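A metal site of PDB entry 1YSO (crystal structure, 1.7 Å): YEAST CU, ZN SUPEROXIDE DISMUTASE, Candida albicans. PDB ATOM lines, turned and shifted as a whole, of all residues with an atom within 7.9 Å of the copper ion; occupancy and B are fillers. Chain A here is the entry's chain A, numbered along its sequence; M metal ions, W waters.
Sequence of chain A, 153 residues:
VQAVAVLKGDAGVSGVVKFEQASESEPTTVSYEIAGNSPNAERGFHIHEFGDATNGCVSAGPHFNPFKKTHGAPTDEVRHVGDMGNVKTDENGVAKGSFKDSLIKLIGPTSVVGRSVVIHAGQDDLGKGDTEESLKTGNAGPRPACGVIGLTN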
ATOM      1  N   GLY A  44       2.161 -12.411 -20.746  1.00  0.00           N
ATOM      2  CA  GLY A  44       1.940 -11.212 -19.926  1.00  0.00           C
ATOM      3  C   GLY A  44       2.717 -10.018 -20.454  1.00  0.00           C
ATOM      4  O   GLY A  44       3.893 -10.149 -20.770  1.00  0.00           O
ATOM      5  N   PHE A  45       2.063  -8.846 -20.442  1.00  0.00           N
ATOM      6  CA  PHE A  45       2.587  -7.630 -21.035  1.00  0.00           C
ATOM      7  C   PHE A  45       2.289  -6.470 -20.093  1.00  0.00           C
ATOM      8  O   PHE A  45       1.097  -6.148 -19.882  1.00  0.00           O
ATOM      9  CB  PHE A  45       1.881  -7.500 -22.361  1.00  0.00           C
ATOM     10  CG  PHE A  45       2.326  -6.416 -23.316  1.00  0.00           C
ATOM     11  CD1 PHE A  45       3.677  -6.161 -23.560  1.00  0.00           C
ATOM     12  CD2 PHE A  45       1.359  -5.663 -23.958  1.00  0.00           C
ATOM     13  CE1 PHE A  45       4.064  -5.187 -24.489  1.00  0.00           C
ATOM     14  CE2 PHE A  45       1.753  -4.696 -24.886  1.00  0.00           C
ATOM     15  CZ  PHE A  45       3.090  -4.443 -25.138  1.00  0.00           C
ATOM     16  N   HIS A  46       3.267  -5.826 -19.471  1.00  0.00           N
ATOM     17  CA  HIS A  46       2.968  -4.777 -18.508  1.00  0.00           C
ATOM     18  C   HIS A  46       3.963  -3.642 -18.539  1.00  0.00           C
ATOM     19  O   HIS A  46       5.079  -3.782 -19.045  1.00  0.00           O
ATOM     20  CB  HIS A  46       3.004  -5.278 -17.065  1.00  0.00           C
ATOM     21  CG  HIS A  46       2.540  -6.717 -16.842  1.00  0.00           C
ATOM     22  ND1 HIS A  46       3.333  -7.705 -16.461  1.00  0.00           N
ATOM     23  CD2 HIS A  46       1.258  -7.194 -17.012  1.00  0.00           C
ATOM     24  CE1 HIS A  46       2.570  -8.775 -16.398  1.00  0.00           C
ATOM     25  NE2 HIS A  46       1.339  -8.451 -16.726  1.00  0.00           N
ATOM     26  N   ILE A  47       3.557  -2.512 -17.943  1.00  0.00           N
ATOM     27  CA  ILE A  47       4.482  -1.424 -17.704  1.00  0.00           C
ATOM     28  C   ILE A  47       4.914  -1.561 -16.256  1.00  0.00           C
ATOM     29  O   ILE A  47       4.099  -1.742 -15.343  1.00  0.00           O
ATOM     30  CB  ILE A  47       3.805  -0.079 -17.936  1.00  0.00           C
ATOM     31  CG1 ILE A  47       3.401  -0.062 -19.416  1.00  0.00           C
ATOM     32  CG2 ILE A  47       4.723   1.084 -17.561  1.00  0.00           C
ATOM     33  CD1 ILE A  47       2.643   1.142 -19.966  1.00  0.00           C
ATOM     34  N   HIS A  48       6.222  -1.592 -16.059  1.00  0.00           N
ATOM     35  CA  HIS A  48       6.848  -1.724 -14.767  1.00  0.00           C
ATOM     36  C   HIS A  48       7.302  -0.342 -14.336  1.00  0.00           C
ATOM     37  O   HIS A  48       7.475   0.568 -15.163  1.00  0.00           O
ATOM     38  CB  HIS A  48       8.012  -2.707 -14.872  1.00  0.00           C
ATOM     39  CG  HIS A  48       7.568  -4.145 -14.828  1.00  0.00           C
ATOM     40  ND1 HIS A  48       7.928  -5.078 -13.983  1.00  0.00           N
ATOM     41  CD2 HIS A  48       6.677  -4.721 -15.697  1.00  0.00           C
ATOM     42  CE1 HIS A  48       7.308  -6.190 -14.297  1.00  0.00           C
ATOM     43  NE2 HIS A  48       6.545  -5.975 -15.329  1.00  0.00           N
ATOM     44  N   GLY A  61      11.742  -3.266 -11.815  1.00  0.00           N
ATOM     45  CA  GLY A  61      10.902  -3.232 -10.616  1.00  0.00           C
ATOM     46  C   GLY A  61       9.510  -3.834 -10.792  1.00  0.00           C
ATOM     47  O   GLY A  61       9.305  -4.605 -11.702  1.00  0.00           O
ATOM     48  N   PRO A  62       8.568  -3.534  -9.900  1.00  0.00           N
ATOM     49  CA  PRO A  62       7.200  -4.050  -9.904  1.00  0.00           C
ATOM     50  C   PRO A  62       6.336  -3.388 -10.969  1.00  0.00           C
ATOM     51  O   PRO A  62       6.773  -2.429 -11.637  1.00  0.00           O
ATOM     52  CB  PRO A  62       6.741  -3.757  -8.502  1.00  0.00           C
ATOM     53  CG  PRO A  62       7.332  -2.383  -8.301  1.00  0.00           C
ATOM     54  CD  PRO A  62       8.754  -2.625  -8.766  1.00  0.00           C
ATOM     55  N   HIS A  63       5.084  -3.849 -11.135  1.00  0.00           N
ATOM     56  CA  HIS A  63       4.140  -3.221 -12.037  1.00  0.00           C
ATOM     57  C   HIS A  63       3.896  -1.786 -11.575  1.00  0.00           C
ATOM     58  O   HIS A  63       3.854  -1.501 -10.367  1.00  0.00           O
ATOM     59  CB  HIS A  63       2.801  -3.925 -12.053  1.00  0.00           C
ATOM     60  CG  HIS A  63       2.825  -5.339 -12.605  1.00  0.00           C
ATOM     61  ND1 HIS A  63       1.802  -6.154 -12.610  1.00  0.00           N
ATOM     62  CD2 HIS A  63       3.898  -5.986 -13.161  1.00  0.00           C
ATOM     63  CE1 HIS A  63       2.206  -7.289 -13.151  1.00  0.00           C
ATOM     64  NE2 HIS A  63       3.466  -7.185 -13.490  1.00  0.00           N
ATOM     65  N   PHE A  64       3.746  -0.882 -12.537  1.00  0.00           N
ATOM     66  CA  PHE A  64       3.523   0.518 -12.223  1.00  0.00           C
ATOM     67  C   PHE A  64       2.122   0.581 -11.615  1.00  0.00           C
ATOM     68  O   PHE A  64       1.112   0.204 -12.226  1.00  0.00           O
ATOM     69  CB  PHE A  64       3.635   1.368 -13.497  1.00  0.00           C
ATOM     70  CG  PHE A  64       3.447   2.866 -13.225  1.00  0.00           C
ATOM     71  CD1 PHE A  64       4.073   3.503 -12.151  1.00  0.00           C
ATOM     72  CD2 PHE A  64       2.632   3.614 -14.089  1.00  0.00           C
ATOM     73  CE1 PHE A  64       3.857   4.868 -11.911  1.00  0.00           C
ATOM     74  CE2 PHE A  64       2.431   4.980 -13.841  1.00  0.00           C
ATOM     75  CZ  PHE A  64       3.050   5.598 -12.761  1.00  0.00           C
ATOM     76  N   HIS A  71      -3.280  -6.478  -8.815  1.00  0.00           N
ATOM     77  CA  HIS A  71      -3.137  -6.869 -10.211  1.00  0.00           C
ATOM     78  C   HIS A  71      -4.461  -7.300 -10.817  1.00  0.00           C
ATOM     79  O   HIS A  71      -5.237  -7.985 -10.152  1.00  0.00           O
ATOM     80  CB  HIS A  71      -2.100  -8.008 -10.249  1.00  0.00           C
ATOM     81  CG  HIS A  71      -1.745  -8.379 -11.670  1.00  0.00           C
ATOM     82  ND1 HIS A  71      -0.993  -7.697 -12.530  1.00  0.00           N
ATOM     83  CD2 HIS A  71      -2.270  -9.469 -12.292  1.00  0.00           C
ATOM     84  CE1 HIS A  71      -1.050  -8.364 -13.662  1.00  0.00           C
ATOM     85  NE2 HIS A  71      -1.817  -9.390 -13.496  1.00  0.00           N
ATOM     86  N   GLY A  82      -0.193  -0.189 -14.922  1.00  0.00           N
ATOM     87  CA  GLY A  82       0.658  -0.867 -15.908  1.00  0.00           C
ATOM     88  C   GLY A  82       0.137  -2.185 -16.476  1.00  0.00           C
ATOM     89  O   GLY A  82       0.797  -2.809 -17.302  1.00  0.00           O
ATOM     90  N   ASP A  83      -1.015  -2.677 -16.049  1.00  0.00           N
ATOM     91  CA  ASP A  83      -1.533  -3.944 -16.517  1.00  0.00           C
ATOM     92  C   ASP A  83      -2.154  -3.856 -17.912  1.00  0.00           C
ATOM     93  O   ASP A  83      -3.203  -3.259 -18.126  1.00  0.00           O
ATOM     94  CB  ASP A  83      -2.572  -4.456 -15.510  1.00  0.00           C
ATOM     95  CG  ASP A  83      -1.989  -4.889 -14.170  1.00  0.00           C
ATOM     96  OD1 ASP A  83      -0.766  -5.069 -14.007  1.00  0.00           O
ATOM     97  OD2 ASP A  83      -2.781  -5.031 -13.250  1.00  0.00           O
ATOM     98  N   GLY A  85      -2.501  -6.894 -19.638  1.00  0.00           N
ATOM     99  CA  GLY A  85      -3.007  -8.219 -19.945  1.00  0.00           C
ATOM    100  C   GLY A  85      -2.021  -9.151 -20.652  1.00  0.00           C
ATOM    101  O   GLY A  85      -0.841  -9.128 -20.323  1.00  0.00           O
ATOM    102  N   SER A 116       9.368   1.316 -17.895  1.00  0.00           N
ATOM    103  CA  SER A 116       9.737   0.195 -18.772  1.00  0.00           C
ATOM    104  C   SER A 116       8.555  -0.643 -19.203  1.00  0.00           C
ATOM    105  O   SER A 116       7.583  -0.772 -18.478  1.00  0.00           O
ATOM    106  CB  SER A 116      10.641  -0.785 -18.101  1.00  0.00           C
ATOM    107  OG  SER A 116      11.904  -0.224 -17.765  1.00  0.00           O
ATOM    108  N   VAL A 117       8.653  -1.225 -20.394  1.00  0.00           N
ATOM    109  CA  VAL A 117       7.651  -2.211 -20.822  1.00  0.00           C
ATOM    110  C   VAL A 117       8.361  -3.544 -20.701  1.00  0.00           C
ATOM    111  O   VAL A 117       9.546  -3.635 -21.081  1.00  0.00           O
ATOM    112  CB  VAL A 117       7.238  -2.074 -22.293  1.00  0.00           C
ATOM    113  CG1 VAL A 117       6.151  -3.086 -22.633  1.00  0.00           C
ATOM    114  CG2 VAL A 117       6.717  -0.680 -22.555  1.00  0.00           C
ATOM    115  N   VAL A 118       7.637  -4.538 -20.214  1.00  0.00           N
ATOM    116  CA  VAL A 118       8.146  -5.887 -20.027  1.00  0.00           C
ATOM    117  C   VAL A 118       7.182  -6.878 -20.677  1.00  0.00           C
ATOM    118  O   VAL A 118       5.969  -6.747 -20.545  1.00  0.00           O
ATOM    119  CB  VAL A 118       8.309  -6.205 -18.502  1.00  0.00           C
ATOM    120  CG1 VAL A 118       8.725  -7.652 -18.278  1.00  0.00           C
ATOM    121  CG2 VAL A 118       9.458  -5.427 -17.924  1.00  0.00           C
ATOM    122  N   ILE A 119       7.764  -7.809 -21.450  1.00  0.00           N
ATOM    123  CA  ILE A 119       7.035  -8.926 -22.044  1.00  0.00           C
ATOM    124  C   ILE A 119       7.551 -10.142 -21.259  1.00  0.00           C
ATOM    125  O   ILE A 119       8.759 -10.359 -21.073  1.00  0.00           O
ATOM    126  CB  ILE A 119       7.342  -9.048 -23.626  1.00  0.00           C
ATOM    127  CG1 ILE A 119       6.581 -10.227 -24.231  1.00  0.00           C
ATOM    128  CG2 ILE A 119       8.815  -9.304 -23.904  1.00  0.00           C
ATOM    129  CD1 ILE A 119       5.062 -10.158 -24.251  1.00  0.00           C
ATOM    130  N   HIS A 120       6.588 -10.913 -20.750  1.00  0.00           N
ATOM    131  CA  HIS A 120       6.874 -12.065 -19.929  1.00  0.00           C
ATOM    132  C   HIS A 120       6.954 -13.367 -20.705  1.00  0.00           C
ATOM    133  O   HIS A 120       6.505 -13.430 -21.845  1.00  0.00           O
ATOM    134  CB  HIS A 120       5.817 -12.229 -18.862  1.00  0.00           C
ATOM    135  CG  HIS A 120       6.048 -11.235 -17.736  1.00  0.00           C
ATOM    136  ND1 HIS A 120       6.810 -11.385 -16.660  1.00  0.00           N
ATOM    137  CD2 HIS A 120       5.464  -9.985 -17.679  1.00  0.00           C
ATOM    138  CE1 HIS A 120       6.717 -10.282 -15.962  1.00  0.00           C
ATOM    139  NE2 HIS A 120       5.911  -9.449 -16.580  1.00  0.00           N
ATOM    140  N   ASP A 124      -0.284 -14.331 -18.099  1.00  0.00           N
ATOM    141  CA  ASP A 124      -0.725 -13.583 -16.932  1.00  0.00           C
ATOM    142  C   ASP A 124      -2.084 -14.163 -16.564  1.00  0.00           C
ATOM    143  O   ASP A 124      -2.999 -14.157 -17.376  1.00  0.00           O
ATOM    144  CB  ASP A 124      -0.818 -12.123 -17.358  1.00  0.00           C
ATOM    145  CG  ASP A 124      -1.219 -11.093 -16.337  1.00  0.00           C
ATOM    146  OD1 ASP A 124      -1.769 -11.472 -15.311  1.00  0.00           O
ATOM    147  OD2 ASP A 124      -1.022  -9.923 -16.584  1.00  0.00           O
ATOM    148  N   LYS A 136      -0.257  -9.850  -7.325  1.00  0.00           N
ATOM    149  CA  LYS A 136       0.895  -8.994  -7.480  1.00  0.00           C
ATOM    150  C   LYS A 136       1.405  -8.984  -8.900  1.00  0.00           C
ATOM    151  O   LYS A 136       1.617  -7.896  -9.437  1.00  0.00           O
ATOM    152  CB  LYS A 136       2.071  -9.426  -6.604  1.00  0.00           C
ATOM    153  CG  LYS A 136       1.868  -9.094  -5.134  1.00  0.00           C
ATOM    154  CD  LYS A 136       3.133  -9.408  -4.332  1.00  0.00           C
ATOM    155  CE  LYS A 136       2.809  -9.163  -2.836  1.00  0.00           C
ATOM    156  NZ  LYS A 136       3.910  -9.540  -1.947  1.00  0.00           N
ATOM    157  N   THR A 137       1.645 -10.141  -9.524  1.00  0.00           N
ATOM    158  CA  THR A 137       2.239 -10.187 -10.852  1.00  0.00           C
ATOM    159  C   THR A 137       1.387 -10.898 -11.883  1.00  0.00           C
ATOM    160  O   THR A 137       1.681 -10.903 -13.079  1.00  0.00           O
ATOM    161  CB  THR A 137       3.612 -10.888 -10.785  1.00  0.00           C
ATOM    162  OG1 THR A 137       3.346 -12.265 -10.442  1.00  0.00           O
ATOM    163  CG2 THR A 137       4.519 -10.317  -9.729  1.00  0.00           C
ATOM    164  N   GLY A 138       0.345 -11.586 -11.421  1.00  0.00           N
ATOM    165  CA  GLY A 138      -0.444 -12.422 -12.320  1.00  0.00           C
ATOM    166  C   GLY A 138       0.324 -13.705 -12.615  1.00  0.00           C
ATOM    167  O   GLY A 138      -0.077 -14.414 -13.523  1.00  0.00           O
ATOM    168  N   ALA A 140       3.026 -14.233 -14.092  1.00  0.00           N
ATOM    169  CA  ALA A 140       3.432 -14.223 -15.490  1.00  0.00           C
ATOM    170  C   ALA A 140       4.850 -14.724 -15.725  1.00  0.00           C
ATOM    171  O   ALA A 140       5.264 -14.886 -16.877  1.00  0.00           O
ATOM    172  CB  ALA A 140       3.290 -12.823 -16.051  1.00  0.00           C
ATOM    173  N   GLY A 141       5.643 -14.947 -14.673  1.00  0.00           N
ATOM    174  CA  GLY A 141       6.937 -15.593 -14.802  1.00  0.00           C
ATOM    175  C   GLY A 141       8.078 -14.681 -15.201  1.00  0.00           C
ATOM    176  O   GLY A 141       8.003 -13.481 -14.991  1.00  0.00           O
ATOM    177  N   PRO A 142       9.151 -15.250 -15.790  1.00  0.00           N
ATOM    178  CA  PRO A 142      10.344 -14.498 -16.181  1.00  0.00           C
ATOM    179  C   PRO A 142      10.064 -13.356 -17.166  1.00  0.00           C
ATOM    180  O   PRO A 142       9.025 -13.282 -17.797  1.00  0.00           O
ATOM    181  CB  PRO A 142      11.275 -15.581 -16.725  1.00  0.00           C
ATOM    182  CG  PRO A 142      10.792 -16.880 -16.112  1.00  0.00           C
ATOM    183  CD  PRO A 142       9.292 -16.677 -16.047  1.00  0.00           C
ATOM    184  N   ARG A 143      11.064 -12.491 -17.371  1.00  0.00           N
ATOM    185  CA  ARG A 143      10.978 -11.295 -18.182  1.00  0.00           C
ATOM    186  C   ARG A 143      12.008 -11.449 -19.281  1.00  0.00           C
ATOM    187  O   ARG A 143      13.134 -11.005 -19.077  1.00  0.00           O
ATOM    188  CB  ARG A 143      11.324 -10.066 -17.311  1.00  0.00           C
ATOM    189  CG  ARG A 143      10.537  -9.947 -16.017  1.00  0.00           C
ATOM    190  CD  ARG A 143      11.038  -8.773 -15.207  1.00  0.00           C
ATOM    191  NE  ARG A 143      10.300  -8.760 -13.971  1.00  0.00           N
ATOM    192  CZ  ARG A 143      10.332  -7.742 -13.104  1.00  0.00           C
ATOM    193  NH1 ARG A 143      11.055  -6.641 -13.318  1.00  0.00           N
ATOM    194  NH2 ARG A 143       9.571  -7.808 -12.021  1.00  0.00           N
HETATM  195 CU    CU M   1       5.202  -7.636 -15.815  1.00  0.00          CU
HETATM  196 ZN    ZN M   2      -0.024  -5.797 -12.431  1.00  0.00          ZN
HETATM  197  O   HOH W   1       5.984  -8.860 -13.007  1.00  0.00           O
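ND1 of His 48 lies within hydrogen-bond range of O of Gly 61. The backbone NH (N) of His 48 lies within hydrogen-bond range of the backbone carbonyl oxygen (O) of Ser 116 (2.9 Å). ND1 of His 120 sits at hydrogen-bond distance from O of Gly 141. NE2 of His 46 lies within hydrogen-bond range of OD2 of Asp 124, 2.8 Å away. O of Pro 142 sits at hydrogen-bond distance from ND1 of His 120, 3.1 Å away. The backbone carbonyl oxygen (O) of His 46 is in hydrogen-bond range of the backbone NH (N) of Val 118 (2.9 Å). The backbone NH of His 120 sits at hydrogen-bond distance from the backbone carbonyl oxygen of Gly 44, 2.8 Å away. NE2 of His 63 lies close to ND1 of His 46 (3.0 Å).
Merely in contact with the copper ion: His 63 (2.9 Å). Of the 26 residues printed, 4 come within 4 Å of the copper ion. The nearest printed residue that does not touch the copper ion is Val 118 (4.3 Å).
ND1 of His 46 binds the copper ion, at 2.0 Å. NE2 of His 120 binds the copper ion. The copper ion is bound by a ring nitrogen (NE2) of His 48 (2.2 Å). The copper ion has three donor atoms within binding distance.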
